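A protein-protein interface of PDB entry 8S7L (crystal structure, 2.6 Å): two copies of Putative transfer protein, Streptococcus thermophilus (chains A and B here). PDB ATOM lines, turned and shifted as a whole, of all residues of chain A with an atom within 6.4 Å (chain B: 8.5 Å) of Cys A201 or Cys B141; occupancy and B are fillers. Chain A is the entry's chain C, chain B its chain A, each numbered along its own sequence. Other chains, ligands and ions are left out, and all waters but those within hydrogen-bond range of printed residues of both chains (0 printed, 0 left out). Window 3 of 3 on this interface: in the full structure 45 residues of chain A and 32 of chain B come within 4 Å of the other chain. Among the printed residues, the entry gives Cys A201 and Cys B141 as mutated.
No position is printed for both chains.
Cys A201 touches just one residue of chain B: Cys B141. Of the printed residues of chain A, Cys B141 touches Ile A199, Val A200 and Cys A201. Of the printed residues of chain A, Phe B139 touches Val A200 (3.5 Å). Of the printed residues of chain B, Val A200 touches Phe B139 and Cys B141. Of the printed residues of chain A, Tyr B101 touches Val A230 (3.5 Å). Of the printed residues of chain A, Val B117 touches Asn A202 (3.4 Å). Of the printed residues of chain B, Val A230 touches Tyr B101 (3.5 Å). The nearest printed residue of chain A that does not touch Tyr B101 is Asn A202 (6.8 Å).
The side-chain hydroxyl (OG1) of Thr A203 is in hydrogen-bond range of the backbone carbonyl oxygen (O) of Cys A201 (2.8 Å). N of Leu B116 is in hydrogen-bond range of O of Tyr B101 (2.9 Å). O of Tyr A183 lies within hydrogen-bond range of N of Val A200 (3.0 Å).
SG of Cys A201 is disulfide-bonded to SG of Cys B141 (2.1 Å). The side-chain sulfur of Cys B141 sits close to the backbone carbonyl oxygen of Ile A199, at 3.4 Å. The side-chain amide nitrogen (ND2) of Asn A202 is in hydrogen-bond range of the backbone carbonyl oxygen (O) of Val B117.
O of Phe B139 touches CG1 of Val A200, 3.5 Å away. Val A200 touches Cys B141. Val A230 touches Tyr B101.
Of the 9 printed residues of chain A, 5 touch a printed residue of chain B. Hydrophobic or aromatic side chains of chain A that line the printed part of chain B: Val A200 and Val A230. Along chain A the printed residues that touch a printed residue of chain B span positions 199 to 230. Of the 17 printed residues of chain B, 4 touch a printed residue of chain A. Hydrophobic or aromatic side chains of chain B within 4 Å of the printed part of chain A: Tyr B101. Along chain B the printed residues that touch a printed residue of chain A span positions 101 to 141.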
ATOM      1  N   TYR A 183       5.342  21.829 -26.475  1.00  0.00           N
ATOM      2  CA  TYR A 183       6.730  21.675 -26.050  1.00  0.00           C
ATOM      3  C   TYR A 183       7.234  22.991 -25.481  1.00  0.00           C
ATOM      4  O   TYR A 183       8.074  22.977 -24.584  1.00  0.00           O
ATOM      5  CB  TYR A 183       7.543  21.112 -27.215  1.00  0.00           C
ATOM      6  CG  TYR A 183       9.053  21.036 -27.058  1.00  0.00           C
ATOM      7  CD1 TYR A 183       9.714  19.953 -26.459  1.00  0.00           C
ATOM      8  CD2 TYR A 183       9.830  22.029 -27.623  1.00  0.00           C
ATOM      9  CE1 TYR A 183      11.099  19.896 -26.394  1.00  0.00           C
ATOM     10  CE2 TYR A 183      11.206  21.991 -27.550  1.00  0.00           C
ATOM     11  CZ  TYR A 183      11.857  20.932 -26.933  1.00  0.00           C
ATOM     12  OH  TYR A 183      13.247  21.035 -26.965  1.00  0.00           O
ATOM     13  N   THR A 184       6.605  24.090 -25.910  1.00  0.00           N
ATOM     14  CA  THR A 184       6.934  25.409 -25.408  1.00  0.00           C
ATOM     15  C   THR A 184       5.912  25.970 -24.420  1.00  0.00           C
ATOM     16  O   THR A 184       6.065  27.126 -24.060  1.00  0.00           O
ATOM     17  CB  THR A 184       7.082  26.354 -26.594  1.00  0.00           C
ATOM     18  OG1 THR A 184       5.754  26.615 -27.029  1.00  0.00           O
ATOM     19  CG2 THR A 184       7.888  25.711 -27.698  1.00  0.00           C
ATOM     20  N   ILE A 199       9.103  20.102 -21.112  1.00  0.00           N
ATOM     21  CA  ILE A 199       8.922  21.336 -21.850  1.00  0.00           C
ATOM     22  C   ILE A 199      10.153  22.201 -21.653  1.00  0.00           C
ATOM     23  O   ILE A 199      10.907  21.992 -20.704  1.00  0.00           O
ATOM     24  CB  ILE A 199       7.675  22.102 -21.377  1.00  0.00           C
ATOM     25  CG1 ILE A 199       7.816  22.533 -19.873  1.00  0.00           C
ATOM     26  CG2 ILE A 199       6.406  21.300 -21.672  1.00  0.00           C
ATOM     27  CD1 ILE A 199       6.707  23.439 -19.361  1.00  0.00           C
ATOM     28  N   VAL A 200      10.234  23.218 -22.521  1.00  0.00           N
ATOM     29  CA  VAL A 200      11.272  24.222 -22.485  1.00  0.00           C
ATOM     30  C   VAL A 200      10.738  25.547 -21.964  1.00  0.00           C
ATOM     31  O   VAL A 200       9.599  25.897 -22.201  1.00  0.00           O
ATOM     32  CB  VAL A 200      11.874  24.401 -23.897  1.00  0.00           C
ATOM     33  CG1 VAL A 200      12.533  23.121 -24.380  1.00  0.00           C
ATOM     34  CG2 VAL A 200      10.875  24.912 -24.929  1.00  0.00           C
ATOM     35  N   CYS A 201      11.633  26.345 -21.388  1.00  0.00           N
ATOM     36  CA  CYS A 201      11.269  27.596 -20.739  1.00  0.00           C
ATOM     37  C   CYS A 201      11.490  28.764 -21.706  1.00  0.00           C
ATOM     38  O   CYS A 201      12.267  28.646 -22.655  1.00  0.00           O
ATOM     39  CB  CYS A 201      12.123  27.721 -19.477  1.00  0.00           C
ATOM     40  SG  CYS A 201      11.643  26.571 -18.151  1.00  0.00           S
ATOM     41  N   ASN A 202      10.813  29.896 -21.447  1.00  0.00           N
ATOM     42  CA  ASN A 202      11.086  31.215 -22.038  1.00  0.00           C
ATOM     43  C   ASN A 202      11.147  31.202 -23.571  1.00  0.00           C
ATOM     44  O   ASN A 202      11.915  31.969 -24.153  1.00  0.00           O
ATOM     45  CB  ASN A 202      12.373  31.873 -21.509  1.00  0.00           C
ATOM     46  CG  ASN A 202      12.465  31.935 -19.998  1.00  0.00           C
ATOM     47  OD1 ASN A 202      11.520  32.347 -19.316  1.00  0.00           O
ATOM     48  ND2 ASN A 202      13.580  31.499 -19.439  1.00  0.00           N
ATOM     49  N   THR A 203      10.317  30.378 -24.229  1.00  0.00           N
ATOM     50  CA  THR A 203      10.457  30.072 -25.652  1.00  0.00           C
ATOM     51  C   THR A 203       9.107  30.213 -26.381  1.00  0.00           C
ATOM     52  O   THR A 203       8.077  29.749 -25.892  1.00  0.00           O
ATOM     53  CB  THR A 203      11.064  28.664 -25.836  1.00  0.00           C
ATOM     54  OG1 THR A 203      12.425  28.608 -25.413  1.00  0.00           O
ATOM     55  CG2 THR A 203      11.238  28.260 -27.291  1.00  0.00           C
ATOM     56  N   THR A 204       9.140  30.820 -27.583  1.00  0.00           N
ATOM     57  CA  THR A 204       8.045  30.746 -28.534  1.00  0.00           C
ATOM     58  C   THR A 204       8.432  29.922 -29.759  1.00  0.00           C
ATOM     59  O   THR A 204       9.436  30.204 -30.427  1.00  0.00           O
ATOM     60  CB  THR A 204       7.658  32.146 -29.008  1.00  0.00           C
ATOM     61  OG1 THR A 204       7.412  32.930 -27.857  1.00  0.00           O
ATOM     62  CG2 THR A 204       6.374  32.149 -29.824  1.00  0.00           C
ATOM     63  N   VAL A 230      13.602  33.034 -28.233  1.00  0.00           N
ATOM     64  CA  VAL A 230      13.908  33.250 -26.830  1.00  0.00           C
ATOM     65  C   VAL A 230      14.382  34.690 -26.726  1.00  0.00           C
ATOM     66  O   VAL A 230      15.377  35.041 -27.399  1.00  0.00           O
ATOM     67  CB  VAL A 230      15.041  32.321 -26.339  1.00  0.00           C
ATOM     68  CG1 VAL A 230      15.202  32.450 -24.840  1.00  0.00           C
ATOM     69  CG2 VAL A 230      14.859  30.868 -26.743  1.00  0.00           C
ATOM     70  N   THR B  96      25.535  19.546 -20.953  1.00  0.00           N
ATOM     71  CA  THR B  96      24.451  20.368 -20.482  1.00  0.00           C
ATOM     72  C   THR B  96      24.962  21.467 -19.566  1.00  0.00           C
ATOM     73  O   THR B  96      25.477  21.153 -18.489  1.00  0.00           O
ATOM     74  CB  THR B  96      23.425  19.480 -19.784  1.00  0.00           C
ATOM     75  OG1 THR B  96      22.961  18.525 -20.741  1.00  0.00           O
ATOM     76  CG2 THR B  96      22.249  20.271 -19.275  1.00  0.00           C
ATOM     77  N   TYR B  97      24.690  22.731 -19.941  1.00  0.00           N
ATOM     78  CA  TYR B  97      25.053  23.870 -19.109  1.00  0.00           C
ATOM     79  C   TYR B  97      23.807  24.500 -18.467  1.00  0.00           C
ATOM     80  O   TYR B  97      22.677  24.170 -18.791  1.00  0.00           O
ATOM     81  CB  TYR B  97      25.868  24.881 -19.937  1.00  0.00           C
ATOM     82  CG  TYR B  97      27.346  24.573 -20.163  1.00  0.00           C
ATOM     83  CD1 TYR B  97      27.798  23.576 -21.028  1.00  0.00           C
ATOM     84  CD2 TYR B  97      28.314  25.377 -19.583  1.00  0.00           C
ATOM     85  CE1 TYR B  97      29.153  23.328 -21.237  1.00  0.00           C
ATOM     86  CE2 TYR B  97      29.671  25.144 -19.760  1.00  0.00           C
ATOM     87  CZ  TYR B  97      30.090  24.107 -20.578  1.00  0.00           C
ATOM     88  OH  TYR B  97      31.424  23.940 -20.697  1.00  0.00           O
ATOM     89  N   LYS B  98      24.078  25.353 -17.487  1.00  0.00           N
ATOM     90  CA  LYS B  98      23.162  26.351 -16.974  1.00  0.00           C
ATOM     91  C   LYS B  98      23.831  27.702 -17.226  1.00  0.00           C
ATOM     92  O   LYS B  98      25.022  27.873 -17.025  1.00  0.00           O
ATOM     93  CB  LYS B  98      22.692  25.926 -15.574  1.00  0.00           C
ATOM     94  CG  LYS B  98      23.498  26.241 -14.388  1.00  0.00           C
ATOM     95  CD  LYS B  98      22.919  25.397 -13.259  1.00  0.00           C
ATOM     96  CE  LYS B  98      23.520  25.750 -11.920  1.00  0.00           C
ATOM     97  NZ  LYS B  98      23.063  24.740 -10.956  1.00  0.00           N
ATOM     98  N   TYR B 101      22.597  35.068 -19.191  1.00  0.00           N
ATOM     99  CA  TYR B 101      23.079  36.007 -20.200  1.00  0.00           C
ATOM    100  C   TYR B 101      22.147  37.215 -20.269  1.00  0.00           C
ATOM    101  O   TYR B 101      21.018  37.120 -19.779  1.00  0.00           O
ATOM    102  CB  TYR B 101      23.172  35.351 -21.573  1.00  0.00           C
ATOM    103  CG  TYR B 101      21.893  34.911 -22.277  1.00  0.00           C
ATOM    104  CD1 TYR B 101      21.314  33.702 -21.988  1.00  0.00           C
ATOM    105  CD2 TYR B 101      21.341  35.634 -23.323  1.00  0.00           C
ATOM    106  CE1 TYR B 101      20.199  33.254 -22.652  1.00  0.00           C
ATOM    107  CE2 TYR B 101      20.222  35.191 -24.014  1.00  0.00           C
ATOM    108  CZ  TYR B 101      19.624  34.008 -23.647  1.00  0.00           C
ATOM    109  OH  TYR B 101      18.481  33.603 -24.267  1.00  0.00           O
ATOM    110  N   LEU B 116      18.225  36.642 -19.009  1.00  0.00           N
ATOM    111  CA  LEU B 116      17.599  35.334 -19.135  1.00  0.00           C
ATOM    112  C   LEU B 116      18.533  34.312 -18.514  1.00  0.00           C
ATOM    113  O   LEU B 116      19.731  34.465 -18.605  1.00  0.00           O
ATOM    114  CB  LEU B 116      17.324  35.012 -20.594  1.00  0.00           C
ATOM    115  CG  LEU B 116      16.610  36.119 -21.394  1.00  0.00           C
ATOM    116  CD1 LEU B 116      16.832  36.192 -22.869  1.00  0.00           C
ATOM    117  CD2 LEU B 116      15.107  36.086 -21.070  1.00  0.00           C
ATOM    118  N   VAL B 117      17.951  33.260 -17.939  1.00  0.00           N
ATOM    119  CA  VAL B 117      18.653  32.035 -17.634  1.00  0.00           C
ATOM    120  C   VAL B 117      18.027  30.914 -18.449  1.00  0.00           C
ATOM    121  O   VAL B 117      16.830  30.959 -18.689  1.00  0.00           O
ATOM    122  CB  VAL B 117      18.570  31.704 -16.146  1.00  0.00           C
ATOM    123  CG1 VAL B 117      19.026  32.910 -15.343  1.00  0.00           C
ATOM    124  CG2 VAL B 117      17.182  31.188 -15.764  1.00  0.00           C
ATOM    125  N   THR B 118      18.819  29.965 -18.908  1.00  0.00           N
ATOM    126  CA  THR B 118      18.276  28.761 -19.493  1.00  0.00           C
ATOM    127  C   THR B 118      19.285  27.621 -19.337  1.00  0.00           C
ATOM    128  O   THR B 118      20.466  27.860 -19.125  1.00  0.00           O
ATOM    129  CB  THR B 118      18.047  29.051 -20.988  1.00  0.00           C
ATOM    130  OG1 THR B 118      17.648  27.844 -21.595  1.00  0.00           O
ATOM    131  CG2 THR B 118      19.316  29.464 -21.705  1.00  0.00           C
ATOM    132  N   GLY B 119      18.819  26.382 -19.567  1.00  0.00           N
ATOM    133  CA  GLY B 119      19.708  25.283 -19.883  1.00  0.00           C
ATOM    134  C   GLY B 119      20.120  25.339 -21.339  1.00  0.00           C
ATOM    135  O   GLY B 119      19.406  25.892 -22.163  1.00  0.00           O
ATOM    136  N   PHE B 120      21.266  24.721 -21.649  1.00  0.00           N
ATOM    137  CA  PHE B 120      21.863  24.858 -22.966  1.00  0.00           C
ATOM    138  C   PHE B 120      22.696  23.617 -23.163  1.00  0.00           C
ATOM    139  O   PHE B 120      23.524  23.300 -22.303  1.00  0.00           O
ATOM    140  CB  PHE B 120      22.771  26.085 -22.992  1.00  0.00           C
ATOM    141  CG  PHE B 120      23.447  26.370 -24.324  1.00  0.00           C
ATOM    142  CD1 PHE B 120      22.698  26.876 -25.385  1.00  0.00           C
ATOM    143  CD2 PHE B 120      24.827  26.213 -24.486  1.00  0.00           C
ATOM    144  CE1 PHE B 120      23.307  27.147 -26.589  1.00  0.00           C
ATOM    145  CE2 PHE B 120      25.426  26.528 -25.692  1.00  0.00           C
ATOM    146  CZ  PHE B 120      24.663  26.975 -26.753  1.00  0.00           C
ATOM    147  N   ASN B 121      22.349  22.880 -24.214  1.00  0.00           N
ATOM    148  CA  ASN B 121      22.816  21.528 -24.426  1.00  0.00           C
ATOM    149  C   ASN B 121      23.573  21.496 -25.745  1.00  0.00           C
ATOM    150  O   ASN B 121      23.079  21.956 -26.765  1.00  0.00           O
ATOM    151  CB  ASN B 121      21.656  20.531 -24.435  1.00  0.00           C
ATOM    152  CG  ASN B 121      20.775  20.719 -23.227  1.00  0.00           C
ATOM    153  OD1 ASN B 121      20.940  20.019 -22.219  1.00  0.00           O
ATOM    154  ND2 ASN B 121      19.907  21.709 -23.286  1.00  0.00           N
ATOM    155  N   TRP B 138      20.781  23.032 -28.270  1.00  0.00           N
ATOM    156  CA  TRP B 138      19.397  23.274 -27.908  1.00  0.00           C
ATOM    157  C   TRP B 138      19.155  23.691 -26.469  1.00  0.00           C
ATOM    158  O   TRP B 138      19.822  23.232 -25.535  1.00  0.00           O
ATOM    159  CB  TRP B 138      18.641  21.985 -28.206  1.00  0.00           C
ATOM    160  CG  TRP B 138      19.051  20.763 -27.430  1.00  0.00           C
ATOM    161  CD1 TRP B 138      18.424  20.265 -26.337  1.00  0.00           C
ATOM    162  CD2 TRP B 138      20.048  19.793 -27.783  1.00  0.00           C
ATOM    163  NE1 TRP B 138      18.978  19.071 -25.966  1.00  0.00           N
ATOM    164  CE2 TRP B 138      19.967  18.744 -26.838  1.00  0.00           C
ATOM    165  CE3 TRP B 138      20.981  19.700 -28.819  1.00  0.00           C
ATOM    166  CZ2 TRP B 138      20.814  17.634 -26.859  1.00  0.00           C
ATOM    167  CZ3 TRP B 138      21.814  18.586 -28.845  1.00  0.00           C
ATOM    168  CH2 TRP B 138      21.731  17.569 -27.882  1.00  0.00           C
ATOM    169  N   PHE B 139      18.056  24.441 -26.293  1.00  0.00           N
ATOM    170  CA  PHE B 139      17.718  25.041 -25.014  1.00  0.00           C
ATOM    171  C   PHE B 139      16.809  24.127 -24.203  1.00  0.00           C
ATOM    172  O   PHE B 139      16.046  23.351 -24.751  1.00  0.00           O
ATOM    173  CB  PHE B 139      17.062  26.401 -25.196  1.00  0.00           C
ATOM    174  CG  PHE B 139      17.985  27.495 -25.702  1.00  0.00           C
ATOM    175  CD1 PHE B 139      18.787  27.274 -26.813  1.00  0.00           C
ATOM    176  CD2 PHE B 139      17.990  28.748 -25.120  1.00  0.00           C
ATOM    177  CE1 PHE B 139      19.575  28.291 -27.321  1.00  0.00           C
ATOM    178  CE2 PHE B 139      18.808  29.747 -25.598  1.00  0.00           C
ATOM    179  CZ  PHE B 139      19.573  29.520 -26.730  1.00  0.00           C
ATOM    180  N   SER B 140      16.927  24.206 -22.877  1.00  0.00           N
ATOM    181  CA  SER B 140      16.081  23.464 -21.972  1.00  0.00           C
ATOM    182  C   SER B 140      15.857  24.289 -20.716  1.00  0.00           C
ATOM    183  O   SER B 140      16.491  25.321 -20.549  1.00  0.00           O
ATOM    184  CB  SER B 140      16.724  22.100 -21.633  1.00  0.00           C
ATOM    185  OG  SER B 140      18.059  22.214 -21.184  1.00  0.00           O
ATOM    186  N   CYS B 141      14.922  23.832 -19.879  1.00  0.00           N
ATOM    187  CA  CYS B 141      14.742  24.364 -18.536  1.00  0.00           C
ATOM    188  C   CYS B 141      15.812  23.796 -17.640  1.00  0.00           C
ATOM    189  O   CYS B 141      16.157  22.658 -17.770  1.00  0.00           O
ATOM    190  CB  CYS B 141      13.446  23.952 -17.841  1.00  0.00           C
ATOM    191  SG  CYS B 141      11.986  24.550 -18.727  1.00  0.00           S
ATOM    192  N   ILE B 142      16.338  24.654 -16.799  1.00  0.00           N
ATOM    193  CA  ILE B 142      17.177  24.282 -15.685  1.00  0.00           C
ATOM    194  C   ILE B 142      16.308  23.534 -14.684  1.00  0.00           C
ATOM    195  O   ILE B 142      15.256  24.010 -14.296  1.00  0.00           O
ATOM    196  CB  ILE B 142      17.790  25.552 -15.076  1.00  0.00           C
ATOM    197  CG1 ILE B 142      18.571  26.362 -16.132  1.00  0.00           C
ATOM    198  CG2 ILE B 142      18.619  25.193 -13.858  1.00  0.00           C
ATOM    199  CD1 ILE B 142      18.730  27.830 -15.792  1.00  0.00           C
ATOM    200  N   GLU B 143      16.701  22.318 -14.339  1.00  0.00           N
ATOM    201  CA  GLU B 143      15.972  21.516 -13.370  1.00  0.00           C
ATOM    202  C   GLU B 143      16.402  21.931 -11.974  1.00  0.00           C
ATOM    203  O   GLU B 143      17.557  22.175 -11.774  1.00  0.00           O
ATOM    204  CB  GLU B 143      16.148  20.016 -13.616  1.00  0.00           C
ATOM    205  CG  GLU B 143      15.232  19.647 -14.771  1.00  0.00           C
ATOM    206  CD  GLU B 143      15.677  18.397 -15.457  1.00  0.00           C
ATOM    207  OE1 GLU B 143      16.666  17.767 -15.045  1.00  0.00           O
ATOM    208  OE2 GLU B 143      15.003  18.111 -16.444  1.00  0.00           O
ATOM    209  N   SER B 144      15.436  22.007 -11.072  1.00  0.00           N
ATOM    210  CA  SER B 144      15.637  22.113  -9.627  1.00  0.00           C
ATOM    211  C   SER B 144      16.348  20.885  -9.071  1.00  0.00           C
ATOM    212  O   SER B 144      16.016  19.791  -9.444  1.00  0.00           O
ATOM    213  CB  SER B 144      14.320  22.250  -8.958  1.00  0.00           C
ATOM    214  OG  SER B 144      14.521  22.164  -7.558  1.00  0.00           O
